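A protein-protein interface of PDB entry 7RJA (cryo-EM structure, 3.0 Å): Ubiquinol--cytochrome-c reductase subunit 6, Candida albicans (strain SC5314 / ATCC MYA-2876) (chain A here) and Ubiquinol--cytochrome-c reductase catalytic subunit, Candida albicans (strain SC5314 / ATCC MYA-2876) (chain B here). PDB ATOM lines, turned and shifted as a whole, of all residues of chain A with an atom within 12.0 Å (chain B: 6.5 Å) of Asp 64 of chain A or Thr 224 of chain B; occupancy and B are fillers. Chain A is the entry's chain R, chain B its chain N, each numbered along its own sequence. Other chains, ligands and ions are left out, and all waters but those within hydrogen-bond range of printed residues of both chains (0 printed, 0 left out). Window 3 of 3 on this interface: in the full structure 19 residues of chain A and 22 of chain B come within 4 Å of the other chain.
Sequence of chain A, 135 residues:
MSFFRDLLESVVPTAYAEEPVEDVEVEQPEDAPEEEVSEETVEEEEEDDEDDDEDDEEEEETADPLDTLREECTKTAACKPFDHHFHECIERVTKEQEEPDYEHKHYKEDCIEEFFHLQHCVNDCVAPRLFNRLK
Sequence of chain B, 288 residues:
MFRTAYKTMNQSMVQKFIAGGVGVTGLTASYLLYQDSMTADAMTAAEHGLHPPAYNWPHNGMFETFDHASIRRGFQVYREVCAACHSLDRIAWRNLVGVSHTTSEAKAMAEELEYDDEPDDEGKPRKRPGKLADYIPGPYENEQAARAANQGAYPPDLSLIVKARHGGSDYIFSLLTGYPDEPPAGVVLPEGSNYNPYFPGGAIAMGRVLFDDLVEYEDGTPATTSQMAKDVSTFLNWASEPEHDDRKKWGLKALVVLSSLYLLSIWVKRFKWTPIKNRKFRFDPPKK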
ATOM      1  N   ALA A  63     -18.427  34.141  23.619  1.00  0.00           N
ATOM      2  CA  ALA A  63     -18.665  32.754  23.997  1.00  0.00           C
ATOM      3  C   ALA A  63     -17.501  32.225  24.825  1.00  0.00           C
ATOM      4  O   ALA A  63     -16.354  32.611  24.611  1.00  0.00           O
ATOM      5  CB  ALA A  63     -18.871  31.895  22.761  1.00  0.00           C
ATOM      6  N   ASP A  64     -17.800  31.340  25.769  1.00  0.00           N
ATOM      7  CA  ASP A  64     -16.751  30.770  26.598  1.00  0.00           C
ATOM      8  C   ASP A  64     -15.811  29.918  25.744  1.00  0.00           C
ATOM      9  O   ASP A  64     -16.260  29.232  24.821  1.00  0.00           O
ATOM     10  CB  ASP A  64     -17.349  29.934  27.730  1.00  0.00           C
ATOM     11  CG  ASP A  64     -18.140  28.747  27.229  1.00  0.00           C
ATOM     12  OD1 ASP A  64     -18.267  28.587  26.000  1.00  0.00           O
ATOM     13  OD2 ASP A  64     -18.633  27.963  28.066  1.00  0.00           O
ATOM     14  N   PRO A  65     -14.503  29.961  26.001  1.00  0.00           N
ATOM     15  CA  PRO A  65     -13.587  29.143  25.193  1.00  0.00           C
ATOM     16  C   PRO A  65     -13.864  27.654  25.267  1.00  0.00           C
ATOM     17  O   PRO A  65     -13.540  26.930  24.319  1.00  0.00           O
ATOM     18  CB  PRO A  65     -12.212  29.491  25.775  1.00  0.00           C
ATOM     19  CG  PRO A  65     -12.377  30.864  26.289  1.00  0.00           C
ATOM     20  CD  PRO A  65     -13.765  30.907  26.855  1.00  0.00           C
ATOM     21  N   LEU A  66     -14.436  27.163  26.366  1.00  0.00           N
ATOM     22  CA  LEU A  66     -14.604  25.721  26.512  1.00  0.00           C
ATOM     23  C   LEU A  66     -15.590  25.165  25.493  1.00  0.00           C
ATOM     24  O   LEU A  66     -15.359  24.095  24.922  1.00  0.00           O
ATOM     25  CB  LEU A  66     -15.057  25.381  27.928  1.00  0.00           C
ATOM     26  CG  LEU A  66     -15.223  23.895  28.236  1.00  0.00           C
ATOM     27  CD1 LEU A  66     -13.893  23.178  28.138  1.00  0.00           C
ATOM     28  CD2 LEU A  66     -15.815  23.726  29.618  1.00  0.00           C
ATOM     29  N   ASP A  67     -16.700  25.864  25.254  1.00  0.00           N
ATOM     30  CA  ASP A  67     -17.680  25.366  24.295  1.00  0.00           C
ATOM     31  C   ASP A  67     -17.088  25.302  22.894  1.00  0.00           C
ATOM     32  O   ASP A  67     -17.243  24.302  22.182  1.00  0.00           O
ATOM     33  CB  ASP A  67     -18.932  26.242  24.310  1.00  0.00           C
ATOM     34  CG  ASP A  67     -19.720  26.110  25.596  1.00  0.00           C
ATOM     35  OD1 ASP A  67     -19.669  25.027  26.214  1.00  0.00           O
ATOM     36  OD2 ASP A  67     -20.398  27.084  25.983  1.00  0.00           O
ATOM     37  N   THR A  68     -16.411  26.370  22.471  1.00  0.00           N
ATOM     38  CA  THR A  68     -15.822  26.373  21.139  1.00  0.00           C
ATOM     39  C   THR A  68     -14.711  25.340  21.019  1.00  0.00           C
ATOM     40  O   THR A  68     -14.563  24.710  19.966  1.00  0.00           O
ATOM     41  CB  THR A  68     -15.310  27.774  20.786  1.00  0.00           C
ATOM     42  OG1 THR A  68     -14.958  27.822  19.398  1.00  0.00           O
ATOM     43  CG2 THR A  68     -14.111  28.162  21.632  1.00  0.00           C
ATOM     44  N   LEU A  69     -13.927  25.139  22.080  1.00  0.00           N
ATOM     45  CA  LEU A  69     -12.915  24.090  22.045  1.00  0.00           C
ATOM     46  C   LEU A  69     -13.553  22.713  21.932  1.00  0.00           C
ATOM     47  O   LEU A  69     -13.061  21.856  21.191  1.00  0.00           O
ATOM     48  CB  LEU A  69     -12.028  24.167  23.285  1.00  0.00           C
ATOM     49  CG  LEU A  69     -11.056  25.342  23.335  1.00  0.00           C
ATOM     50  CD1 LEU A  69     -10.356  25.381  24.672  1.00  0.00           C
ATOM     51  CD2 LEU A  69     -10.038  25.245  22.214  1.00  0.00           C
ATOM     52  N   ARG A  70     -14.645  22.475  22.660  1.00  0.00           N
ATOM     53  CA  ARG A  70     -15.341  21.202  22.531  1.00  0.00           C
ATOM     54  C   ARG A  70     -15.844  21.003  21.111  1.00  0.00           C
ATOM     55  O   ARG A  70     -15.695  19.919  20.534  1.00  0.00           O
ATOM     56  CB  ARG A  70     -16.509  21.130  23.512  1.00  0.00           C
ATOM     57  CG  ARG A  70     -16.206  20.388  24.797  1.00  0.00           C
ATOM     58  CD  ARG A  70     -17.115  20.850  25.920  1.00  0.00           C
ATOM     59  NE  ARG A  70     -16.702  20.326  27.215  1.00  0.00           N
ATOM     60  CZ  ARG A  70     -17.229  20.700  28.374  1.00  0.00           C
ATOM     61  NH1 ARG A  70     -18.205  21.590  28.434  1.00  0.00           N
ATOM     62  NH2 ARG A  70     -16.768  20.163  29.498  1.00  0.00           N
ATOM     63  N   GLU A  71     -16.440  22.042  20.528  1.00  0.00           N
ATOM     64  CA  GLU A  71     -16.942  21.928  19.164  1.00  0.00           C
ATOM     65  C   GLU A  71     -15.808  21.624  18.197  1.00  0.00           C
ATOM     66  O   GLU A  71     -15.939  20.768  17.316  1.00  0.00           O
ATOM     67  CB  GLU A  71     -17.666  23.211  18.761  1.00  0.00           C
ATOM     68  CG  GLU A  71     -18.935  23.467  19.552  1.00  0.00           C
ATOM     69  CD  GLU A  71     -20.012  22.441  19.271  1.00  0.00           C
ATOM     70  OE1 GLU A  71     -20.066  21.929  18.133  1.00  0.00           O
ATOM     71  OE2 GLU A  71     -20.802  22.142  20.191  1.00  0.00           O
ATOM     72  N   GLU A  72     -14.674  22.306  18.358  1.00  0.00           N
ATOM     73  CA  GLU A  72     -13.533  22.050  17.489  1.00  0.00           C
ATOM     74  C   GLU A  72     -13.036  20.619  17.639  1.00  0.00           C
ATOM     75  O   GLU A  72     -12.737  19.949  16.645  1.00  0.00           O
ATOM     76  CB  GLU A  72     -12.411  23.039  17.797  1.00  0.00           C
ATOM     77  CG  GLU A  72     -11.203  22.906  16.891  1.00  0.00           C
ATOM     78  CD  GLU A  72     -10.136  23.935  17.193  1.00  0.00           C
ATOM     79  OE1 GLU A  72     -10.335  24.742  18.126  1.00  0.00           O
ATOM     80  OE2 GLU A  72      -9.097  23.939  16.500  1.00  0.00           O
ATOM     81  N   CYS A  73     -12.948  20.130  18.877  1.00  0.00           N
ATOM     82  CA  CYS A  73     -12.362  18.815  19.114  1.00  0.00           C
ATOM     83  C   CYS A  73     -13.274  17.701  18.613  1.00  0.00           C
ATOM     84  O   CYS A  73     -12.805  16.736  17.998  1.00  0.00           O
ATOM     85  CB  CYS A  73     -12.058  18.645  20.599  1.00  0.00           C
ATOM     86  SG  CYS A  73     -10.785  19.775  21.195  1.00  0.00           S
ATOM     87  N   VAL A 126      -9.037  19.102  24.713  1.00  0.00           N
ATOM     88  CA  VAL A 126      -9.290  20.430  25.268  1.00  0.00           C
ATOM     89  C   VAL A 126      -8.327  20.735  26.408  1.00  0.00           C
ATOM     90  O   VAL A 126      -7.867  21.875  26.553  1.00  0.00           O
ATOM     91  CB  VAL A 126     -10.752  20.570  25.731  1.00  0.00           C
ATOM     92  CG1 VAL A 126     -11.712  20.267  24.598  1.00  0.00           C
ATOM     93  CG2 VAL A 126     -11.016  19.692  26.931  1.00  0.00           C
ATOM     94  N   ARG A 129      -5.153  22.868  25.919  1.00  0.00           N
ATOM     95  CA  ARG A 129      -5.375  24.141  25.249  1.00  0.00           C
ATOM     96  C   ARG A 129      -6.322  25.071  25.992  1.00  0.00           C
ATOM     97  O   ARG A 129      -6.324  26.272  25.710  1.00  0.00           O
ATOM     98  CB  ARG A 129      -5.936  23.907  23.842  1.00  0.00           C
ATOM     99  CG  ARG A 129      -5.073  23.031  22.948  1.00  0.00           C
ATOM    100  CD  ARG A 129      -5.931  22.175  22.034  1.00  0.00           C
ATOM    101  NE  ARG A 129      -6.752  22.983  21.141  1.00  0.00           N
ATOM    102  CZ  ARG A 129      -6.287  23.676  20.111  1.00  0.00           C
ATOM    103  NH1 ARG A 129      -5.001  23.678  19.803  1.00  0.00           N
ATOM    104  NH2 ARG A 129      -7.135  24.383  19.370  1.00  0.00           N
ATOM    105  N   LEU A 130      -7.120  24.557  26.926  1.00  0.00           N
ATOM    106  CA  LEU A 130      -8.201  25.356  27.492  1.00  0.00           C
ATOM    107  C   LEU A 130      -7.669  26.592  28.208  1.00  0.00           C
ATOM    108  O   LEU A 130      -8.097  27.718  27.933  1.00  0.00           O
ATOM    109  CB  LEU A 130      -9.036  24.502  28.444  1.00  0.00           C
ATOM    110  CG  LEU A 130     -10.190  25.227  29.135  1.00  0.00           C
ATOM    111  CD1 LEU A 130     -11.174  25.766  28.120  1.00  0.00           C
ATOM    112  CD2 LEU A 130     -10.883  24.299  30.109  1.00  0.00           C
ATOM    113  N   PHE A 131      -6.727  26.404  29.131  1.00  0.00           N
ATOM    114  CA  PHE A 131      -6.311  27.510  29.984  1.00  0.00           C
ATOM    115  C   PHE A 131      -5.445  28.534  29.267  1.00  0.00           C
ATOM    116  O   PHE A 131      -5.211  29.610  29.825  1.00  0.00           O
ATOM    117  CB  PHE A 131      -5.573  26.980  31.213  1.00  0.00           C
ATOM    118  CG  PHE A 131      -6.467  26.305  32.219  1.00  0.00           C
ATOM    119  CD1 PHE A 131      -7.830  26.193  32.008  1.00  0.00           C
ATOM    120  CD2 PHE A 131      -5.939  25.800  33.389  1.00  0.00           C
ATOM    121  CE1 PHE A 131      -8.639  25.582  32.936  1.00  0.00           C
ATOM    122  CE2 PHE A 131      -6.747  25.190  34.318  1.00  0.00           C
ATOM    123  CZ  PHE A 131      -8.097  25.081  34.091  1.00  0.00           C
ATOM    124  N   ASN A 132      -4.961  28.240  28.061  1.00  0.00           N
ATOM    125  CA  ASN A 132      -4.302  29.282  27.288  1.00  0.00           C
ATOM    126  C   ASN A 132      -5.288  30.338  26.809  1.00  0.00           C
ATOM    127  O   ASN A 132      -4.867  31.436  26.433  1.00  0.00           O
ATOM    128  CB  ASN A 132      -3.565  28.675  26.096  1.00  0.00           C
ATOM    129  CG  ASN A 132      -2.359  27.867  26.515  1.00  0.00           C
ATOM    130  OD1 ASN A 132      -1.690  28.195  27.492  1.00  0.00           O
ATOM    131  ND2 ASN A 132      -2.069  26.807  25.771  1.00  0.00           N
ATOM    132  N   ARG A 133      -6.584  30.031  26.820  1.00  0.00           N
ATOM    133  CA  ARG A 133      -7.605  30.993  26.435  1.00  0.00           C
ATOM    134  C   ARG A 133      -8.067  31.864  27.594  1.00  0.00           C
ATOM    135  O   ARG A 133      -8.751  32.865  27.361  1.00  0.00           O
ATOM    136  CB  ARG A 133      -8.819  30.269  25.847  1.00  0.00           C
ATOM    137  CG  ARG A 133      -8.669  29.859  24.391  1.00  0.00           C
ATOM    138  CD  ARG A 133      -7.481  28.937  24.187  1.00  0.00           C
ATOM    139  NE  ARG A 133      -7.585  28.182  22.944  1.00  0.00           N
ATOM    140  CZ  ARG A 133      -6.563  27.607  22.324  1.00  0.00           C
ATOM    141  NH1 ARG A 133      -5.331  27.681  22.805  1.00  0.00           N
ATOM    142  NH2 ARG A 133      -6.781  26.939  21.197  1.00  0.00           N
ATOM    143  N   LEU A 134      -7.711  31.513  28.826  1.00  0.00           N
ATOM    144  CA  LEU A 134      -8.170  32.248  30.001  1.00  0.00           C
ATOM    145  C   LEU A 134      -7.010  32.924  30.720  1.00  0.00           C
ATOM    146  O   LEU A 134      -7.177  33.464  31.813  1.00  0.00           O
ATOM    147  CB  LEU A 134      -8.901  31.312  30.964  1.00  0.00           C
ATOM    148  CG  LEU A 134      -9.770  30.231  30.322  1.00  0.00           C
ATOM    149  CD1 LEU A 134     -10.355  29.316  31.376  1.00  0.00           C
ATOM    150  CD2 LEU A 134     -10.874  30.868  29.509  1.00  0.00           C
ATOM    151  N   ARG B 208     -26.501  22.544  37.074  1.00  0.00           N
ATOM    152  CA  ARG B 208     -25.616  23.609  36.625  1.00  0.00           C
ATOM    153  C   ARG B 208     -25.952  24.924  37.311  1.00  0.00           C
ATOM    154  O   ARG B 208     -27.119  25.296  37.445  1.00  0.00           O
ATOM    155  CB  ARG B 208     -25.715  23.778  35.112  1.00  0.00           C
ATOM    156  CG  ARG B 208     -24.712  24.760  34.556  1.00  0.00           C
ATOM    157  CD  ARG B 208     -24.731  24.790  33.045  1.00  0.00           C
ATOM    158  NE  ARG B 208     -23.817  25.800  32.526  1.00  0.00           N
ATOM    159  CZ  ARG B 208     -23.384  25.848  31.274  1.00  0.00           C
ATOM    160  NH1 ARG B 208     -23.758  24.951  30.377  1.00  0.00           N
ATOM    161  NH2 ARG B 208     -22.553  26.822  30.914  1.00  0.00           N
ATOM    162  N   LEU B 210     -23.113  27.745  37.141  1.00  0.00           N
ATOM    163  CA  LEU B 210     -22.311  28.753  36.460  1.00  0.00           C
ATOM    164  C   LEU B 210     -22.863  28.998  35.062  1.00  0.00           C
ATOM    165  O   LEU B 210     -22.938  28.074  34.245  1.00  0.00           O
ATOM    166  CB  LEU B 210     -20.853  28.311  36.383  1.00  0.00           C
ATOM    167  CG  LEU B 210     -20.171  27.944  37.698  1.00  0.00           C
ATOM    168  CD1 LEU B 210     -18.704  27.661  37.455  1.00  0.00           C
ATOM    169  CD2 LEU B 210     -20.330  29.050  38.722  1.00  0.00           C
ATOM    170  N   PHE B 211     -23.241  30.243  34.788  1.00  0.00           N
ATOM    171  CA  PHE B 211     -23.680  30.658  33.467  1.00  0.00           C
ATOM    172  C   PHE B 211     -22.919  31.911  33.062  1.00  0.00           C
ATOM    173  O   PHE B 211     -22.439  32.671  33.905  1.00  0.00           O
ATOM    174  CB  PHE B 211     -25.189  30.917  33.423  1.00  0.00           C
ATOM    175  CG  PHE B 211     -26.018  29.696  33.685  1.00  0.00           C
ATOM    176  CD1 PHE B 211     -26.238  28.768  32.684  1.00  0.00           C
ATOM    177  CD2 PHE B 211     -26.584  29.481  34.926  1.00  0.00           C
ATOM    178  CE1 PHE B 211     -27.001  27.644  32.917  1.00  0.00           C
ATOM    179  CE2 PHE B 211     -27.351  28.359  35.165  1.00  0.00           C
ATOM    180  CZ  PHE B 211     -27.559  27.439  34.158  1.00  0.00           C
ATOM    181  N   ASP B 212     -22.821  32.119  31.753  1.00  0.00           N
ATOM    182  CA  ASP B 212     -21.991  33.191  31.228  1.00  0.00           C
ATOM    183  C   ASP B 212     -22.441  34.542  31.769  1.00  0.00           C
ATOM    184  O   ASP B 212     -23.636  34.825  31.875  1.00  0.00           O
ATOM    185  CB  ASP B 212     -22.045  33.191  29.703  1.00  0.00           C
ATOM    186  CG  ASP B 212     -21.410  31.956  29.103  1.00  0.00           C
ATOM    187  OD1 ASP B 212     -20.195  31.758  29.304  1.00  0.00           O
ATOM    188  OD2 ASP B 212     -22.126  31.180  28.437  1.00  0.00           O
ATOM    189  N   ASP B 213     -21.465  35.378  32.120  1.00  0.00           N
ATOM    190  CA  ASP B 213     -21.723  36.730  32.605  1.00  0.00           C
ATOM    191  C   ASP B 213     -22.586  36.725  33.862  1.00  0.00           C
ATOM    192  O   ASP B 213     -23.329  37.674  34.122  1.00  0.00           O
ATOM    193  CB  ASP B 213     -22.375  37.589  31.519  1.00  0.00           C
ATOM    194  CG  ASP B 213     -21.489  37.760  30.303  1.00  0.00           C
ATOM    195  OD1 ASP B 213     -20.249  37.722  30.459  1.00  0.00           O
ATOM    196  OD2 ASP B 213     -22.030  37.931  29.190  1.00  0.00           O
ATOM    197  N   LEU B 214     -22.496  35.656  34.655  1.00  0.00           N
ATOM    198  CA  LEU B 214     -23.259  35.592  35.895  1.00  0.00           C
ATOM    199  C   LEU B 214     -22.683  36.497  36.972  1.00  0.00           C
ATOM    200  O   LEU B 214     -23.412  36.888  37.889  1.00  0.00           O
ATOM    201  CB  LEU B 214     -23.314  34.151  36.403  1.00  0.00           C
ATOM    202  CG  LEU B 214     -23.977  33.941  37.764  1.00  0.00           C
ATOM    203  CD1 LEU B 214     -25.428  34.377  37.723  1.00  0.00           C
ATOM    204  CD2 LEU B 214     -23.874  32.490  38.181  1.00  0.00           C
ATOM    205  N   TYR B 217     -16.864  40.663  37.338  1.00  0.00           N
ATOM    206  CA  TYR B 217     -15.605  40.605  38.063  1.00  0.00           C
ATOM    207  C   TYR B 217     -15.075  42.005  38.341  1.00  0.00           C
ATOM    208  O   TYR B 217     -15.251  42.931  37.545  1.00  0.00           O
ATOM    209  CB  TYR B 217     -14.574  39.804  37.271  1.00  0.00           C
ATOM    210  CG  TYR B 217     -14.669  38.307  37.458  1.00  0.00           C
ATOM    211  CD1 TYR B 217     -14.849  37.752  38.715  1.00  0.00           C
ATOM    212  CD2 TYR B 217     -14.583  37.451  36.375  1.00  0.00           C
ATOM    213  CE1 TYR B 217     -14.935  36.393  38.885  1.00  0.00           C
ATOM    214  CE2 TYR B 217     -14.668  36.092  36.536  1.00  0.00           C
ATOM    215  CZ  TYR B 217     -14.844  35.569  37.792  1.00  0.00           C
ATOM    216  OH  TYR B 217     -14.929  34.210  37.951  1.00  0.00           O
ATOM    217  N   THR B 221     -12.473  41.345  34.285  1.00  0.00           N
ATOM    218  CA  THR B 221     -12.225  40.080  33.617  1.00  0.00           C
ATOM    219  C   THR B 221     -13.535  39.523  33.066  1.00  0.00           C
ATOM    220  O   THR B 221     -14.560  39.565  33.751  1.00  0.00           O
ATOM    221  CB  THR B 221     -11.603  39.078  34.589  1.00  0.00           C
ATOM    222  OG1 THR B 221     -10.249  39.451  34.867  1.00  0.00           O
ATOM    223  CG2 THR B 221     -11.626  37.670  34.022  1.00  0.00           C
ATOM    224  N   PRO B 222     -13.543  39.004  31.838  1.00  0.00           N
ATOM    225  CA  PRO B 222     -14.761  38.363  31.335  1.00  0.00           C
ATOM    226  C   PRO B 222     -15.169  37.200  32.224  1.00  0.00           C
ATOM    227  O   PRO B 222     -14.329  36.482  32.769  1.00  0.00           O
ATOM    228  CB  PRO B 222     -14.368  37.893  29.930  1.00  0.00           C
ATOM    229  CG  PRO B 222     -12.880  37.855  29.938  1.00  0.00           C
ATOM    230  CD  PRO B 222     -12.466  38.972  30.836  1.00  0.00           C
ATOM    231  N   ALA B 223     -16.479  37.016  32.363  1.00  0.00           N
ATOM    232  CA  ALA B 223     -17.011  36.070  33.335  1.00  0.00           C
ATOM    233  C   ALA B 223     -17.615  34.852  32.655  1.00  0.00           C
ATOM    234  O   ALA B 223     -18.655  34.348  33.086  1.00  0.00           O
ATOM    235  CB  ALA B 223     -18.057  36.750  34.214  1.00  0.00           C
ATOM    236  N   THR B 224     -16.971  34.373  31.595  1.00  0.00           N
ATOM    237  CA  THR B 224     -17.423  33.168  30.913  1.00  0.00           C
ATOM    238  C   THR B 224     -17.545  32.026  31.913  1.00  0.00           C
ATOM    239  O   THR B 224     -16.817  31.992  32.909  1.00  0.00           O
ATOM    240  CB  THR B 224     -16.454  32.796  29.791  1.00  0.00           C
ATOM    241  OG1 THR B 224     -15.160  32.531  30.344  1.00  0.00           O
ATOM    242  CG2 THR B 224     -16.346  33.926  28.779  1.00  0.00           C
ATOM    243  N   THR B 225     -18.463  31.090  31.667  1.00  0.00           N
ATOM    244  CA  THR B 225     -18.649  29.992  32.609  1.00  0.00           C
ATOM    245  C   THR B 225     -17.362  29.209  32.812  1.00  0.00           C
ATOM    246  O   THR B 225     -17.074  28.768  33.929  1.00  0.00           O
ATOM    247  CB  THR B 225     -19.756  29.057  32.127  1.00  0.00           C
ATOM    248  OG1 THR B 225     -20.042  28.091  33.145  1.00  0.00           O
ATOM    249  CG2 THR B 225     -19.337  28.338  30.860  1.00  0.00           C
ATOM    250  N   SER B 226     -16.574  29.029  31.753  1.00  0.00           N
ATOM    251  CA  SER B 226     -15.289  28.360  31.905  1.00  0.00           C
ATOM    252  C   SER B 226     -14.377  29.145  32.831  1.00  0.00           C
ATOM    253  O   SER B 226     -13.749  28.575  33.732  1.00  0.00           O
ATOM    254  CB  SER B 226     -14.634  28.194  30.540  1.00  0.00           C
ATOM    255  OG  SER B 226     -15.507  27.518  29.660  1.00  0.00           O
ATOM    256  N   GLN B 227     -14.307  30.460  32.636  1.00  0.00           N
ATOM    257  CA  GLN B 227     -13.448  31.268  33.484  1.00  0.00           C
ATOM    258  C   GLN B 227     -13.913  31.197  34.928  1.00  0.00           C
ATOM    259  O   GLN B 227     -13.095  31.039  35.838  1.00  0.00           O
ATOM    260  CB  GLN B 227     -13.435  32.714  32.989  1.00  0.00           C
ATOM    261  CG  GLN B 227     -12.652  33.674  33.861  1.00  0.00           C
ATOM    262  CD  GLN B 227     -11.165  33.478  33.710  1.00  0.00           C
ATOM    263  OE1 GLN B 227     -10.537  32.793  34.514  1.00  0.00           O
ATOM    264  NE2 GLN B 227     -10.584  34.110  32.704  1.00  0.00           N
ATOM    265  N   MET B 228     -15.226  31.286  35.153  1.00  0.00           N
ATOM    266  CA  MET B 228     -15.748  31.242  36.514  1.00  0.00           C
ATOM    267  C   MET B 228     -15.453  29.905  37.174  1.00  0.00           C
ATOM    268  O   MET B 228     -15.107  29.855  38.359  1.00  0.00           O
ATOM    269  CB  MET B 228     -17.251  31.501  36.505  1.00  0.00           C
ATOM    270  CG  MET B 228     -17.632  32.896  36.079  1.00  0.00           C
ATOM    271  SD  MET B 228     -19.414  33.092  36.016  1.00  0.00           S
ATOM    272  CE  MET B 228     -19.778  33.047  37.763  1.00  0.00           C
ATOM    273  N   ALA B 229     -15.601  28.810  36.429  1.00  0.00           N
ATOM    274  CA  ALA B 229     -15.245  27.510  36.976  1.00  0.00           C
ATOM    275  C   ALA B 229     -13.775  27.475  37.352  1.00  0.00           C
ATOM    276  O   ALA B 229     -13.408  26.927  38.395  1.00  0.00           O
ATOM    277  CB  ALA B 229     -15.568  26.405  35.973  1.00  0.00           C
ATOM    278  N   ASP B 231     -11.876  30.048  38.251  1.00  0.00           N
ATOM    279  CA  ASP B 231     -11.663  30.852  39.452  1.00  0.00           C
ATOM    280  C   ASP B 231     -12.147  30.130  40.698  1.00  0.00           C
ATOM    281  O   ASP B 231     -11.447  30.102  41.716  1.00  0.00           O
ATOM    282  CB  ASP B 231     -12.346  32.214  39.339  1.00  0.00           C
ATOM    283  CG  ASP B 231     -12.030  32.927  38.044  1.00  0.00           C
ATOM    284  OD1 ASP B 231     -12.867  32.895  37.124  1.00  0.00           O
ATOM    285  OD2 ASP B 231     -10.928  33.503  37.946  1.00  0.00           O
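CB of Asp 64 of chain A touches OD1 of Asp 212 of chain B, 3.7 Å away. Asp 64 of chain A touches Thr 224 of chain B. Asp 64 of chain A touches Thr 225 of chain B (OD2 to CG2, 2.9 Å). Asp 64 of chain A touches Ser 226 of chain B. Leu 134 of chain A touches Gln 227 of chain B.
OG of Ser 226 of chain B lies close to N of Leu 66 of chain A (3.5 Å).
O of Leu 210 of chain B is in hydrogen-bond range of OG1 of Thr 225 of chain B (3.1 Å). The side-chain carboxylate (OD1) of Asp 212 of chain B sits at hydrogen-bond distance from the backbone NH (N) of Thr 225 of chain B, 3.0 Å away. The side-chain hydroxyl of Thr 224 of chain B lies close to the backbone NH of Gln 227 of chain B, 3.2 Å away. The side-chain amide oxygen (OE1) of Gln 227 of chain B sits close to the side-chain carboxylate (OD1) of Asp 231 of chain B. OD1 of Asp 64 of chain A sits close to N of Asp 67 of chain A (3.2 Å).
Asp 64 of chain A touches just these residues of chain B: Asp 212, Thr 224, Thr 225 and Ser 226. Thr 224 of chain B touches one residue of chain A. Asp 212 of chain B touches just one residue of chain A: Asp 64 (3.7 Å). Asp 213 of chain B touches none of the printed residues of chain A. No residue of chain A comes within 4 Å of Pro 222 of chain B. No residue of chain A comes within 4 Å of Ala 223 of chain B. Thr 225 of chain B touches just one residue of chain A: Asp 64. Ser 226 of chain B touches just these residues of chain A: Asp 64 and Leu 66. Gln 227 of chain B touches just one residue of chain A: Leu 134 (3.6 Å). Printed residues of chain B within 4 Å of Leu 134 of chain A: Gln 227 (3.6 Å). Printed residues of chain B within 4 Å of Leu 66 of chain A: Ser 226. Leu 69 of chain A touches none of the printed residues of chain B. Ala 63 of chain A touches none of the printed residues of chain B.
Printed residues of chain B that touch a printed residue of chain A: Asp 212, Thr 224, Thr 225, Ser 226 and Gln 227.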
